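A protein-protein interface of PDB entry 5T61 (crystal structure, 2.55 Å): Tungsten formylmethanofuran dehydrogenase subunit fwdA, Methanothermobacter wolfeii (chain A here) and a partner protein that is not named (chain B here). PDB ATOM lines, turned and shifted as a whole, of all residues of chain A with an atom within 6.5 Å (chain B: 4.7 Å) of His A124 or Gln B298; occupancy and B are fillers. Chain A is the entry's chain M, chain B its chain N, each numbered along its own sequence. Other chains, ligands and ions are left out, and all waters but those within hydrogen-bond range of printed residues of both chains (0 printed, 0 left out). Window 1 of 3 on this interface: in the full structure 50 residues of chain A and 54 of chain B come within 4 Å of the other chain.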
ATOM      1  N   ALA A  61      -1.242  -7.413  31.220  1.00  0.00           N
ATOM      2  CA  ALA A  61      -2.021  -6.336  30.611  1.00  0.00           C
ATOM      3  C   ALA A  61      -1.922  -6.422  29.096  1.00  0.00           C
ATOM      4  O   ALA A  61      -0.835  -6.250  28.535  1.00  0.00           O
ATOM      5  CB  ALA A  61      -1.532  -4.973  31.105  1.00  0.00           C
ATOM      6  N   GLY A  62      -3.050  -6.664  28.436  1.00  0.00           N
ATOM      7  CA  GLY A  62      -3.077  -6.648  26.988  1.00  0.00           C
ATOM      8  C   GLY A  62      -4.028  -7.643  26.358  1.00  0.00           C
ATOM      9  O   GLY A  62      -4.750  -8.360  27.058  1.00  0.00           O
ATOM     10  N   ALA A  63      -4.021  -7.694  25.023  1.00  0.00           N
ATOM     11  CA  ALA A  63      -4.962  -8.537  24.290  1.00  0.00           C
ATOM     12  C   ALA A  63      -4.720 -10.010  24.585  1.00  0.00           C
ATOM     13  O   ALA A  63      -5.653 -10.762  24.889  1.00  0.00           O
ATOM     14  CB  ALA A  63      -4.846  -8.264  22.791  1.00  0.00           C
ATOM     15  N   LYS A  64      -3.465 -10.436  24.474  1.00  0.00           N
ATOM     16  CA  LYS A  64      -3.094 -11.823  24.716  1.00  0.00           C
ATOM     17  C   LYS A  64      -3.499 -12.260  26.120  1.00  0.00           C
ATOM     18  O   LYS A  64      -3.962 -13.390  26.325  1.00  0.00           O
ATOM     19  CB  LYS A  64      -1.585 -11.936  24.500  1.00  0.00           C
ATOM     20  CG  LYS A  64      -0.917 -13.285  24.613  1.00  0.00           C
ATOM     21  CD  LYS A  64       0.566 -13.083  24.956  1.00  0.00           C
ATOM     22  CE  LYS A  64       1.201 -11.861  24.257  1.00  0.00           C
ATOM     23  NZ  LYS A  64       0.977 -11.749  22.781  1.00  0.00           N
ATOM     24  N   ASN A  66      -6.014 -10.889  28.045  1.00  0.00           N
ATOM     25  CA  ASN A  66      -7.454 -10.890  28.292  1.00  0.00           C
ATOM     26  C   ASN A  66      -8.174 -12.009  27.546  1.00  0.00           C
ATOM     27  O   ASN A  66      -9.250 -12.441  27.977  1.00  0.00           O
ATOM     28  CB  ASN A  66      -8.076  -9.543  27.930  1.00  0.00           C
ATOM     29  CG  ASN A  66      -9.267  -9.210  28.808  1.00  0.00           C
ATOM     30  OD1 ASN A  66      -9.268  -9.508  30.005  1.00  0.00           O
ATOM     31  ND2 ASN A  66     -10.297  -8.621  28.217  1.00  0.00           N
ATOM     32  N   VAL A  67      -7.618 -12.471  26.424  1.00  0.00           N
ATOM     33  CA  VAL A  67      -8.133 -13.688  25.803  1.00  0.00           C
ATOM     34  C   VAL A  67      -8.009 -14.864  26.760  1.00  0.00           C
ATOM     35  O   VAL A  67      -8.934 -15.674  26.894  1.00  0.00           O
ATOM     36  CB  VAL A  67      -7.409 -13.959  24.471  1.00  0.00           C
ATOM     37  CG1 VAL A  67      -7.840 -15.288  23.911  1.00  0.00           C
ATOM     38  CG2 VAL A  67      -7.747 -12.872  23.470  1.00  0.00           C
ATOM     39  N   ARG A  69      -8.006 -14.629  29.997  1.00  0.00           N
ATOM     40  CA  ARG A  69      -9.054 -14.408  30.986  1.00  0.00           C
ATOM     41  C   ARG A  69     -10.419 -14.792  30.430  1.00  0.00           C
ATOM     42  O   ARG A  69     -11.187 -15.513  31.075  1.00  0.00           O
ATOM     43  CB  ARG A  69      -9.075 -12.945  31.439  1.00  0.00           C
ATOM     44  CG  ARG A  69      -7.806 -12.393  32.063  1.00  0.00           C
ATOM     45  CD  ARG A  69      -8.098 -11.014  32.649  1.00  0.00           C
ATOM     46  NE  ARG A  69      -6.901 -10.297  33.080  1.00  0.00           N
ATOM     47  CZ  ARG A  69      -6.338  -9.304  32.402  1.00  0.00           C
ATOM     48  NH1 ARG A  69      -6.857  -8.910  31.248  1.00  0.00           N
ATOM     49  NH2 ARG A  69      -5.256  -8.703  32.875  1.00  0.00           N
ATOM     50  N   MET A  70     -10.738 -14.323  29.221  1.00  0.00           N
ATOM     51  CA  MET A  70     -12.099 -14.475  28.719  1.00  0.00           C
ATOM     52  C   MET A  70     -12.434 -15.931  28.417  1.00  0.00           C
ATOM     53  O   MET A  70     -13.552 -16.384  28.690  1.00  0.00           O
ATOM     54  CB  MET A  70     -12.310 -13.596  27.484  1.00  0.00           C
ATOM     55  CG  MET A  70     -13.716 -13.697  26.908  1.00  0.00           C
ATOM     56  SD  MET A  70     -13.965 -12.771  25.380  1.00  0.00           S
ATOM     57  CE  MET A  70     -13.604 -11.106  25.938  1.00  0.00           C
ATOM     58  N   MET A 117       3.698  -6.603  24.092  1.00  0.00           N
ATOM     59  CA  MET A 117       2.582  -5.790  23.612  1.00  0.00           C
ATOM     60  C   MET A 117       2.601  -5.646  22.093  1.00  0.00           C
ATOM     61  O   MET A 117       3.567  -5.089  21.542  1.00  0.00           O
ATOM     62  CB  MET A 117       2.606  -4.412  24.272  1.00  0.00           C
ATOM     63  CG  MET A 117       1.519  -3.479  23.774  1.00  0.00           C
ATOM     64  SD  MET A 117       1.430  -1.935  24.698  1.00  0.00           S
ATOM     65  CE  MET A 117       3.034  -1.225  24.371  1.00  0.00           C
ATOM     66  N   LEU A 120      -0.233  -2.430  17.461  1.00  0.00           N
ATOM     67  CA  LEU A 120      -1.563  -2.030  17.014  1.00  0.00           C
ATOM     68  C   LEU A 120      -2.590  -2.143  18.133  1.00  0.00           C
ATOM     69  O   LEU A 120      -3.614  -1.448  18.114  1.00  0.00           O
ATOM     70  CB  LEU A 120      -1.976  -2.884  15.814  1.00  0.00           C
ATOM     71  CG  LEU A 120      -3.394  -2.745  15.260  1.00  0.00           C
ATOM     72  CD1 LEU A 120      -3.564  -1.407  14.552  1.00  0.00           C
ATOM     73  CD2 LEU A 120      -3.714  -3.897  14.317  1.00  0.00           C
ATOM     74  N   LEU A 121      -2.325  -2.992  19.125  1.00  0.00           N
ATOM     75  CA  LEU A 121      -3.225  -3.218  20.246  1.00  0.00           C
ATOM     76  C   LEU A 121      -2.764  -2.501  21.512  1.00  0.00           C
ATOM     77  O   LEU A 121      -3.162  -2.890  22.614  1.00  0.00           O
ATOM     78  CB  LEU A 121      -3.356  -4.720  20.505  1.00  0.00           C
ATOM     79  CG  LEU A 121      -3.582  -5.574  19.251  1.00  0.00           C
ATOM     80  CD1 LEU A 121      -3.618  -7.057  19.592  1.00  0.00           C
ATOM     81  CD2 LEU A 121      -4.845  -5.158  18.511  1.00  0.00           C
ATOM     82  N   ALA A 122      -1.910  -1.481  21.376  1.00  0.00           N
ATOM     83  CA  ALA A 122      -1.269  -0.879  22.543  1.00  0.00           C
ATOM     84  C   ALA A 122      -2.264  -0.171  23.457  1.00  0.00           C
ATOM     85  O   ALA A 122      -2.098  -0.188  24.682  1.00  0.00           O
ATOM     86  CB  ALA A 122      -0.175   0.092  22.099  1.00  0.00           C
ATOM     87  N   ARG A 123      -3.288   0.476  22.888  1.00  0.00           N
ATOM     88  CA  ARG A 123      -4.307   1.113  23.722  1.00  0.00           C
ATOM     89  C   ARG A 123      -4.904   0.115  24.700  1.00  0.00           C
ATOM     90  O   ARG A 123      -5.207   0.456  25.850  1.00  0.00           O
ATOM     91  CB  ARG A 123      -5.411   1.728  22.861  1.00  0.00           C
ATOM     92  CG  ARG A 123      -5.218   3.200  22.556  1.00  0.00           C
ATOM     93  CD  ARG A 123      -6.271   3.679  21.575  1.00  0.00           C
ATOM     94  NE  ARG A 123      -6.110   3.040  20.275  1.00  0.00           N
ATOM     95  CZ  ARG A 123      -5.239   3.431  19.349  1.00  0.00           C
ATOM     96  NH1 ARG A 123      -5.163   2.782  18.196  1.00  0.00           N
ATOM     97  NH2 ARG A 123      -4.440   4.459  19.582  1.00  0.00           N
ATOM     98  N   HIS A 124      -5.083  -1.125  24.247  1.00  0.00           N
ATOM     99  CA  HIS A 124      -5.632  -2.175  25.094  1.00  0.00           C
ATOM    100  C   HIS A 124      -4.774  -2.378  26.336  1.00  0.00           C
ATOM    101  O   HIS A 124      -5.287  -2.413  27.461  1.00  0.00           O
ATOM    102  CB  HIS A 124      -5.734  -3.463  24.274  1.00  0.00           C
ATOM    103  CG  HIS A 124      -6.478  -4.566  24.952  1.00  0.00           C
ATOM    104  ND1 HIS A 124      -6.960  -5.659  24.265  1.00  0.00           N
ATOM    105  CD2 HIS A 124      -6.849  -4.737  26.242  1.00  0.00           C
ATOM    106  CE1 HIS A 124      -7.583  -6.464  25.106  1.00  0.00           C
ATOM    107  NE2 HIS A 124      -7.529  -5.929  26.312  1.00  0.00           N
ATOM    108  N   THR A 125      -3.458  -2.523  26.149  1.00  0.00           N
ATOM    109  CA  THR A 125      -2.552  -2.706  27.280  1.00  0.00           C
ATOM    110  C   THR A 125      -2.641  -1.537  28.256  1.00  0.00           C
ATOM    111  O   THR A 125      -2.744  -1.729  29.473  1.00  0.00           O
ATOM    112  CB  THR A 125      -1.117  -2.873  26.784  1.00  0.00           C
ATOM    113  OG1 THR A 125      -0.996  -4.096  26.048  1.00  0.00           O
ATOM    114  CG2 THR A 125      -0.151  -2.904  27.956  1.00  0.00           C
ATOM    115  N   HIS A 126      -2.593  -0.310  27.733  1.00  0.00           N
ATOM    116  CA  HIS A 126      -2.598   0.866  28.595  1.00  0.00           C
ATOM    117  C   HIS A 126      -3.932   1.046  29.306  1.00  0.00           C
ATOM    118  O   HIS A 126      -3.971   1.591  30.415  1.00  0.00           O
ATOM    119  CB  HIS A 126      -2.244   2.102  27.773  1.00  0.00           C
ATOM    120  CG  HIS A 126      -0.823   2.118  27.301  1.00  0.00           C
ATOM    121  ND1 HIS A 126       0.241   2.283  28.160  1.00  0.00           N
ATOM    122  CD2 HIS A 126      -0.289   1.962  26.066  1.00  0.00           C
ATOM    123  CE1 HIS A 126       1.370   2.247  27.474  1.00  0.00           C
ATOM    124  NE2 HIS A 126       1.075   2.052  26.201  1.00  0.00           N
ATOM    125  N   GLU A 127      -5.030   0.614  28.686  1.00  0.00           N
ATOM    126  CA  GLU A 127      -6.321   0.667  29.361  1.00  0.00           C
ATOM    127  C   GLU A 127      -6.370  -0.297  30.540  1.00  0.00           C
ATOM    128  O   GLU A 127      -6.934   0.022  31.593  1.00  0.00           O
ATOM    129  CB  GLU A 127      -7.437   0.357  28.368  1.00  0.00           C
ATOM    130  CG  GLU A 127      -7.797   1.532  27.488  1.00  0.00           C
ATOM    131  CD  GLU A 127      -9.123   1.345  26.792  1.00  0.00           C
ATOM    132  OE1 GLU A 127      -9.337   0.281  26.176  1.00  0.00           O
ATOM    133  OE2 GLU A 127      -9.951   2.274  26.860  1.00  0.00           O
ATOM    134  N   GLU A 128      -5.797  -1.492  30.377  1.00  0.00           N
ATOM    135  CA  GLU A 128      -5.770  -2.446  31.478  1.00  0.00           C
ATOM    136  C   GLU A 128      -4.813  -1.997  32.576  1.00  0.00           C
ATOM    137  O   GLU A 128      -5.060  -2.260  33.759  1.00  0.00           O
ATOM    138  CB  GLU A 128      -5.409  -3.833  30.949  1.00  0.00           C
ATOM    139  CG  GLU A 128      -6.438  -4.351  29.941  1.00  0.00           C
ATOM    140  CD  GLU A 128      -6.368  -5.849  29.697  1.00  0.00           C
ATOM    141  OE1 GLU A 128      -5.637  -6.549  30.428  1.00  0.00           O
ATOM    142  OE2 GLU A 128      -7.015  -6.317  28.737  1.00  0.00           O
ATOM    143  N   PHE A 129      -3.731  -1.304  32.205  1.00  0.00           N
ATOM    144  CA  PHE A 129      -2.824  -0.739  33.200  1.00  0.00           C
ATOM    145  C   PHE A 129      -3.544   0.253  34.104  1.00  0.00           C
ATOM    146  O   PHE A 129      -3.301   0.289  35.316  1.00  0.00           O
ATOM    147  CB  PHE A 129      -1.643  -0.054  32.509  1.00  0.00           C
ATOM    148  CG  PHE A 129      -0.488  -0.965  32.207  1.00  0.00           C
ATOM    149  CD1 PHE A 129      -0.196  -2.038  33.032  1.00  0.00           C
ATOM    150  CD2 PHE A 129       0.318  -0.734  31.104  1.00  0.00           C
ATOM    151  CE1 PHE A 129       0.879  -2.865  32.761  1.00  0.00           C
ATOM    152  CE2 PHE A 129       1.389  -1.560  30.826  1.00  0.00           C
ATOM    153  CZ  PHE A 129       1.669  -2.627  31.655  1.00  0.00           C
ATOM    154  N   TYR A 557      -4.535   8.082  27.528  1.00  0.00           N
ATOM    155  CA  TYR A 557      -4.335   6.722  28.005  1.00  0.00           C
ATOM    156  C   TYR A 557      -3.193   6.622  29.006  1.00  0.00           C
ATOM    157  O   TYR A 557      -2.988   5.549  29.584  1.00  0.00           O
ATOM    158  CB  TYR A 557      -4.098   5.782  26.820  1.00  0.00           C
ATOM    159  CG  TYR A 557      -5.314   5.634  25.929  1.00  0.00           C
ATOM    160  CD1 TYR A 557      -6.317   4.723  26.239  1.00  0.00           C
ATOM    161  CD2 TYR A 557      -5.474   6.423  24.797  1.00  0.00           C
ATOM    162  CE1 TYR A 557      -7.436   4.587  25.433  1.00  0.00           C
ATOM    163  CE2 TYR A 557      -6.591   6.297  23.990  1.00  0.00           C
ATOM    164  CZ  TYR A 557      -7.568   5.377  24.312  1.00  0.00           C
ATOM    165  OH  TYR A 557      -8.681   5.249  23.511  1.00  0.00           O
ATOM    166  N   THR B 294     -17.689  -5.567  21.327  1.00  0.00           N
ATOM    167  CA  THR B 294     -16.416  -6.166  21.720  1.00  0.00           C
ATOM    168  C   THR B 294     -15.774  -5.398  22.867  1.00  0.00           C
ATOM    169  O   THR B 294     -15.164  -5.997  23.760  1.00  0.00           O
ATOM    170  CB  THR B 294     -15.467  -6.223  20.520  1.00  0.00           C
ATOM    171  OG1 THR B 294     -16.104  -6.905  19.432  1.00  0.00           O
ATOM    172  CG2 THR B 294     -14.185  -6.945  20.882  1.00  0.00           C
ATOM    173  N   GLY B 295     -15.902  -4.070  22.859  1.00  0.00           N
ATOM    174  CA  GLY B 295     -15.275  -3.270  23.899  1.00  0.00           C
ATOM    175  C   GLY B 295     -15.805  -3.580  25.285  1.00  0.00           C
ATOM    176  O   GLY B 295     -15.045  -3.599  26.256  1.00  0.00           O
ATOM    177  N   PHE B 296     -17.115  -3.809  25.406  1.00  0.00           N
ATOM    178  CA  PHE B 296     -17.654  -4.164  26.714  1.00  0.00           C
ATOM    179  C   PHE B 296     -17.091  -5.494  27.191  1.00  0.00           C
ATOM    180  O   PHE B 296     -16.632  -5.610  28.334  1.00  0.00           O
ATOM    181  CB  PHE B 296     -19.177  -4.234  26.702  1.00  0.00           C
ATOM    182  CG  PHE B 296     -19.746  -4.694  28.016  1.00  0.00           C
ATOM    183  CD1 PHE B 296     -19.912  -6.046  28.290  1.00  0.00           C
ATOM    184  CD2 PHE B 296     -20.064  -3.777  29.002  1.00  0.00           C
ATOM    185  CE1 PHE B 296     -20.409  -6.467  29.508  1.00  0.00           C
ATOM    186  CE2 PHE B 296     -20.569  -4.193  30.221  1.00  0.00           C
ATOM    187  CZ  PHE B 296     -20.741  -5.540  30.474  1.00  0.00           C
ATOM    188  N   ASN B 297     -17.131  -6.515  26.331  1.00  0.00           N
ATOM    189  CA  ASN B 297     -16.647  -7.828  26.739  1.00  0.00           C
ATOM    190  C   ASN B 297     -15.183  -7.774  27.142  1.00  0.00           C
ATOM    191  O   ASN B 297     -14.762  -8.520  28.033  1.00  0.00           O
ATOM    192  CB  ASN B 297     -16.847  -8.850  25.616  1.00  0.00           C
ATOM    193  CG  ASN B 297     -18.309  -9.033  25.233  1.00  0.00           C
ATOM    194  OD1 ASN B 297     -18.677  -8.894  24.069  1.00  0.00           O
ATOM    195  ND2 ASN B 297     -19.139  -9.374  26.209  1.00  0.00           N
ATOM    196  N   GLN B 298     -14.404  -6.887  26.521  1.00  0.00           N
ATOM    197  CA  GLN B 298     -13.021  -6.682  26.939  1.00  0.00           C
ATOM    198  C   GLN B 298     -12.956  -6.061  28.328  1.00  0.00           C
ATOM    199  O   GLN B 298     -12.312  -6.603  29.235  1.00  0.00           O
ATOM    200  CB  GLN B 298     -12.290  -5.804  25.923  1.00  0.00           C
ATOM    201  CG  GLN B 298     -12.064  -6.450  24.564  1.00  0.00           C
ATOM    202  CD  GLN B 298     -11.091  -7.611  24.611  1.00  0.00           C
ATOM    203  OE1 GLN B 298     -10.363  -7.789  25.586  1.00  0.00           O
ATOM    204  NE2 GLN B 298     -11.060  -8.399  23.543  1.00  0.00           N
ATOM    205  N   VAL B 299     -13.620  -4.917  28.511  1.00  0.00           N
ATOM    206  CA  VAL B 299     -13.575  -4.211  29.790  1.00  0.00           C
ATOM    207  C   VAL B 299     -14.085  -5.106  30.909  1.00  0.00           C
ATOM    208  O   VAL B 299     -13.437  -5.260  31.952  1.00  0.00           O
ATOM    209  CB  VAL B 299     -14.387  -2.906  29.714  1.00  0.00           C
ATOM    210  CG1 VAL B 299     -14.601  -2.339  31.107  1.00  0.00           C
ATOM    211  CG2 VAL B 299     -13.708  -1.898  28.810  1.00  0.00           C
ATOM    212  N   CYS B 300     -15.263  -5.703  30.710  1.00  0.00           N
ATOM    213  CA  CYS B 300     -15.854  -6.538  31.748  1.00  0.00           C
ATOM    214  C   CYS B 300     -14.961  -7.730  32.068  1.00  0.00           C
ATOM    215  O   CYS B 300     -14.827  -8.118  33.235  1.00  0.00           O
ATOM    216  CB  CYS B 300     -17.244  -7.004  31.315  1.00  0.00           C
ATOM    217  SG  CYS B 300     -18.188  -7.857  32.596  1.00  0.00           S
ATOM    218  N   THR B 301     -14.325  -8.314  31.049  1.00  0.00           N
ATOM    219  CA  THR B 301     -13.426  -9.434  31.301  1.00  0.00           C
ATOM    220  C   THR B 301     -12.228  -8.995  32.131  1.00  0.00           C
ATOM    221  O   THR B 301     -11.874  -9.647  33.118  1.00  0.00           O
ATOM    222  CB  THR B 301     -12.956 -10.071  29.993  1.00  0.00           C
ATOM    223  OG1 THR B 301     -14.071 -10.645  29.303  1.00  0.00           O
ATOM    224  CG2 THR B 301     -11.959 -11.174  30.283  1.00  0.00           C
ATOM    225  N   TRP B 302     -11.590  -7.884  31.753  1.00  0.00           N
ATOM    226  CA  TRP B 302     -10.348  -7.553  32.440  1.00  0.00           C
ATOM    227  C   TRP B 302     -10.615  -6.996  33.834  1.00  0.00           C
ATOM    228  O   TRP B 302      -9.763  -7.122  34.719  1.00  0.00           O
ATOM    229  CB  TRP B 302      -9.481  -6.599  31.596  1.00  0.00           C
ATOM    230  CG  TRP B 302      -9.744  -5.101  31.631  1.00  0.00           C
ATOM    231  CD1 TRP B 302      -9.784  -4.297  32.738  1.00  0.00           C
ATOM    232  CD2 TRP B 302      -9.914  -4.227  30.503  1.00  0.00           C
ATOM    233  NE1 TRP B 302      -9.996  -2.993  32.372  1.00  0.00           N
ATOM    234  CE2 TRP B 302     -10.080  -2.921  31.008  1.00  0.00           C
ATOM    235  CE3 TRP B 302      -9.958  -4.425  29.119  1.00  0.00           C
ATOM    236  CZ2 TRP B 302     -10.290  -1.820  30.179  1.00  0.00           C
ATOM    237  CZ3 TRP B 302     -10.167  -3.327  28.296  1.00  0.00           C
ATOM    238  CH2 TRP B 302     -10.325  -2.042  28.831  1.00  0.00           C
ATOM    239  N   TYR B 394     -13.734  -1.052  20.376  1.00  0.00           N
ATOM    240  CA  TYR B 394     -12.998  -2.243  19.954  1.00  0.00           C
ATOM    241  C   TYR B 394     -13.652  -2.856  18.725  1.00  0.00           C
ATOM    242  O   TYR B 394     -14.831  -3.221  18.758  1.00  0.00           O
ATOM    243  CB  TYR B 394     -12.915  -3.275  21.077  1.00  0.00           C
ATOM    244  CG  TYR B 394     -11.808  -3.014  22.070  1.00  0.00           C
ATOM    245  CD1 TYR B 394     -11.953  -2.065  23.072  1.00  0.00           C
ATOM    246  CD2 TYR B 394     -10.617  -3.724  22.005  1.00  0.00           C
ATOM    247  CE1 TYR B 394     -10.946  -1.832  23.978  1.00  0.00           C
ATOM    248  CE2 TYR B 394      -9.604  -3.498  22.906  1.00  0.00           C
ATOM    249  CZ  TYR B 394      -9.772  -2.552  23.892  1.00  0.00           C
ATOM    250  OH  TYR B 394      -8.767  -2.318  24.798  1.00  0.00           O
ATOM    251  N   PRO B 400      -8.203  -1.872  18.983  1.00  0.00           N
ATOM    252  CA  PRO B 400      -8.741  -0.684  19.664  1.00  0.00           C
ATOM    253  C   PRO B 400      -8.539   0.582  18.837  1.00  0.00           C
ATOM    254  O   PRO B 400      -7.444   0.844  18.332  1.00  0.00           O
ATOM    255  CB  PRO B 400      -7.940  -0.632  20.971  1.00  0.00           C
ATOM    256  CG  PRO B 400      -6.651  -1.339  20.657  1.00  0.00           C
ATOM    257  CD  PRO B 400      -6.874  -2.261  19.487  1.00  0.00           C
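The backbone NH of Gly A62 sits at hydrogen-bond distance from the side-chain carboxylate of Glu A128. The guanidinium group of Arg A69 is in hydrogen-bond range of the side-chain amide oxygen of Asn A66, 2.8 Å away. NH1 of Arg A69 is in salt-bridge range of OE1 of Glu A128 (2.8 Å). A ring nitrogen (NE2) of His A124 lies within hydrogen-bond range of the side-chain carboxylate (OE2) of Glu A128 (2.5 Å). The side-chain hydroxyl (OG1) of Thr B301 lies within hydrogen-bond range of the backbone carbonyl oxygen (O) of Asn B297, at 2.6 Å.
Hydrophobic or aromatic side chains of chain B that line the printed part of chain A: Trp B302, Tyr B394 and Pro B400. Along chain B the printed residues that touch a printed residue of chain A span positions 297 to 400. Hydrophobic or aromatic side chains of chain A within 4 Å of the printed part of chain B: Met A70, Leu A121 and His A124. Along chain A the printed residues that touch a printed residue of chain B span positions 66 to 128. Among the printed residues, no Asp or Glu carboxylate lies within 4 Å of a Lys or Arg side-chain nitrogen of the other chain.
Printed residues of chain B within 4 Å of His A124: Gln B298 (3.1 Å), Tyr B394 (3.2 Å) and Pro B400 (3.9 Å). Gln B298 touches two residues of chain A. Printed residues of chain B within 4 Å of Met A70: Asn B297 (3.5 Å) and Thr B301 (3.4 Å). Printed residues of chain B within 4 Å of Arg A123: Pro B400 (3.0 Å). Of the printed residues of chain B, Leu A120 touches Pro B400 (3.6 Å).
ND2 of Asn A66 is in hydrogen-bond range of OE1 of Gln B298 (2.8 Å). The side-chain amide oxygen (OD1) of Asn A66 lies close to the backbone NH (N) of Trp B302 (3.3 Å). O of Pro B400 sits at hydrogen-bond distance from NH1 of Arg A123 (3.0 Å). The side-chain amide oxygen (OE1) of Gln B298 lies close to a ring nitrogen (NE2) of His A124, 3.5 Å away. OE1 of Glu A127 sits at hydrogen-bond distance from OH of Tyr B394 (3.0 Å).
OD1 of Asn A66 touches CG2 of Thr B301, at 3.2 Å. CB of Arg A69 touches CG2 of Thr B301, 3.6 Å away. CE of Met A70 touches O of Asn B297, 3.5 Å away. CE of Met A70 touches OG1 of Thr B301, at 3.4 Å. Leu A120 touches Pro B400. Leu A121 touches Pro B400. Tyr B394 touches His A124 (OH to CA, 3.2 Å). His A124 touches Pro B400 (N to CG, 3.9 Å). Glu A127 touches Trp B302 (OE1 to CH2, 3.7 Å). OE2 of Glu A128 touches CE3 of Trp B302, at 3.5 Å.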
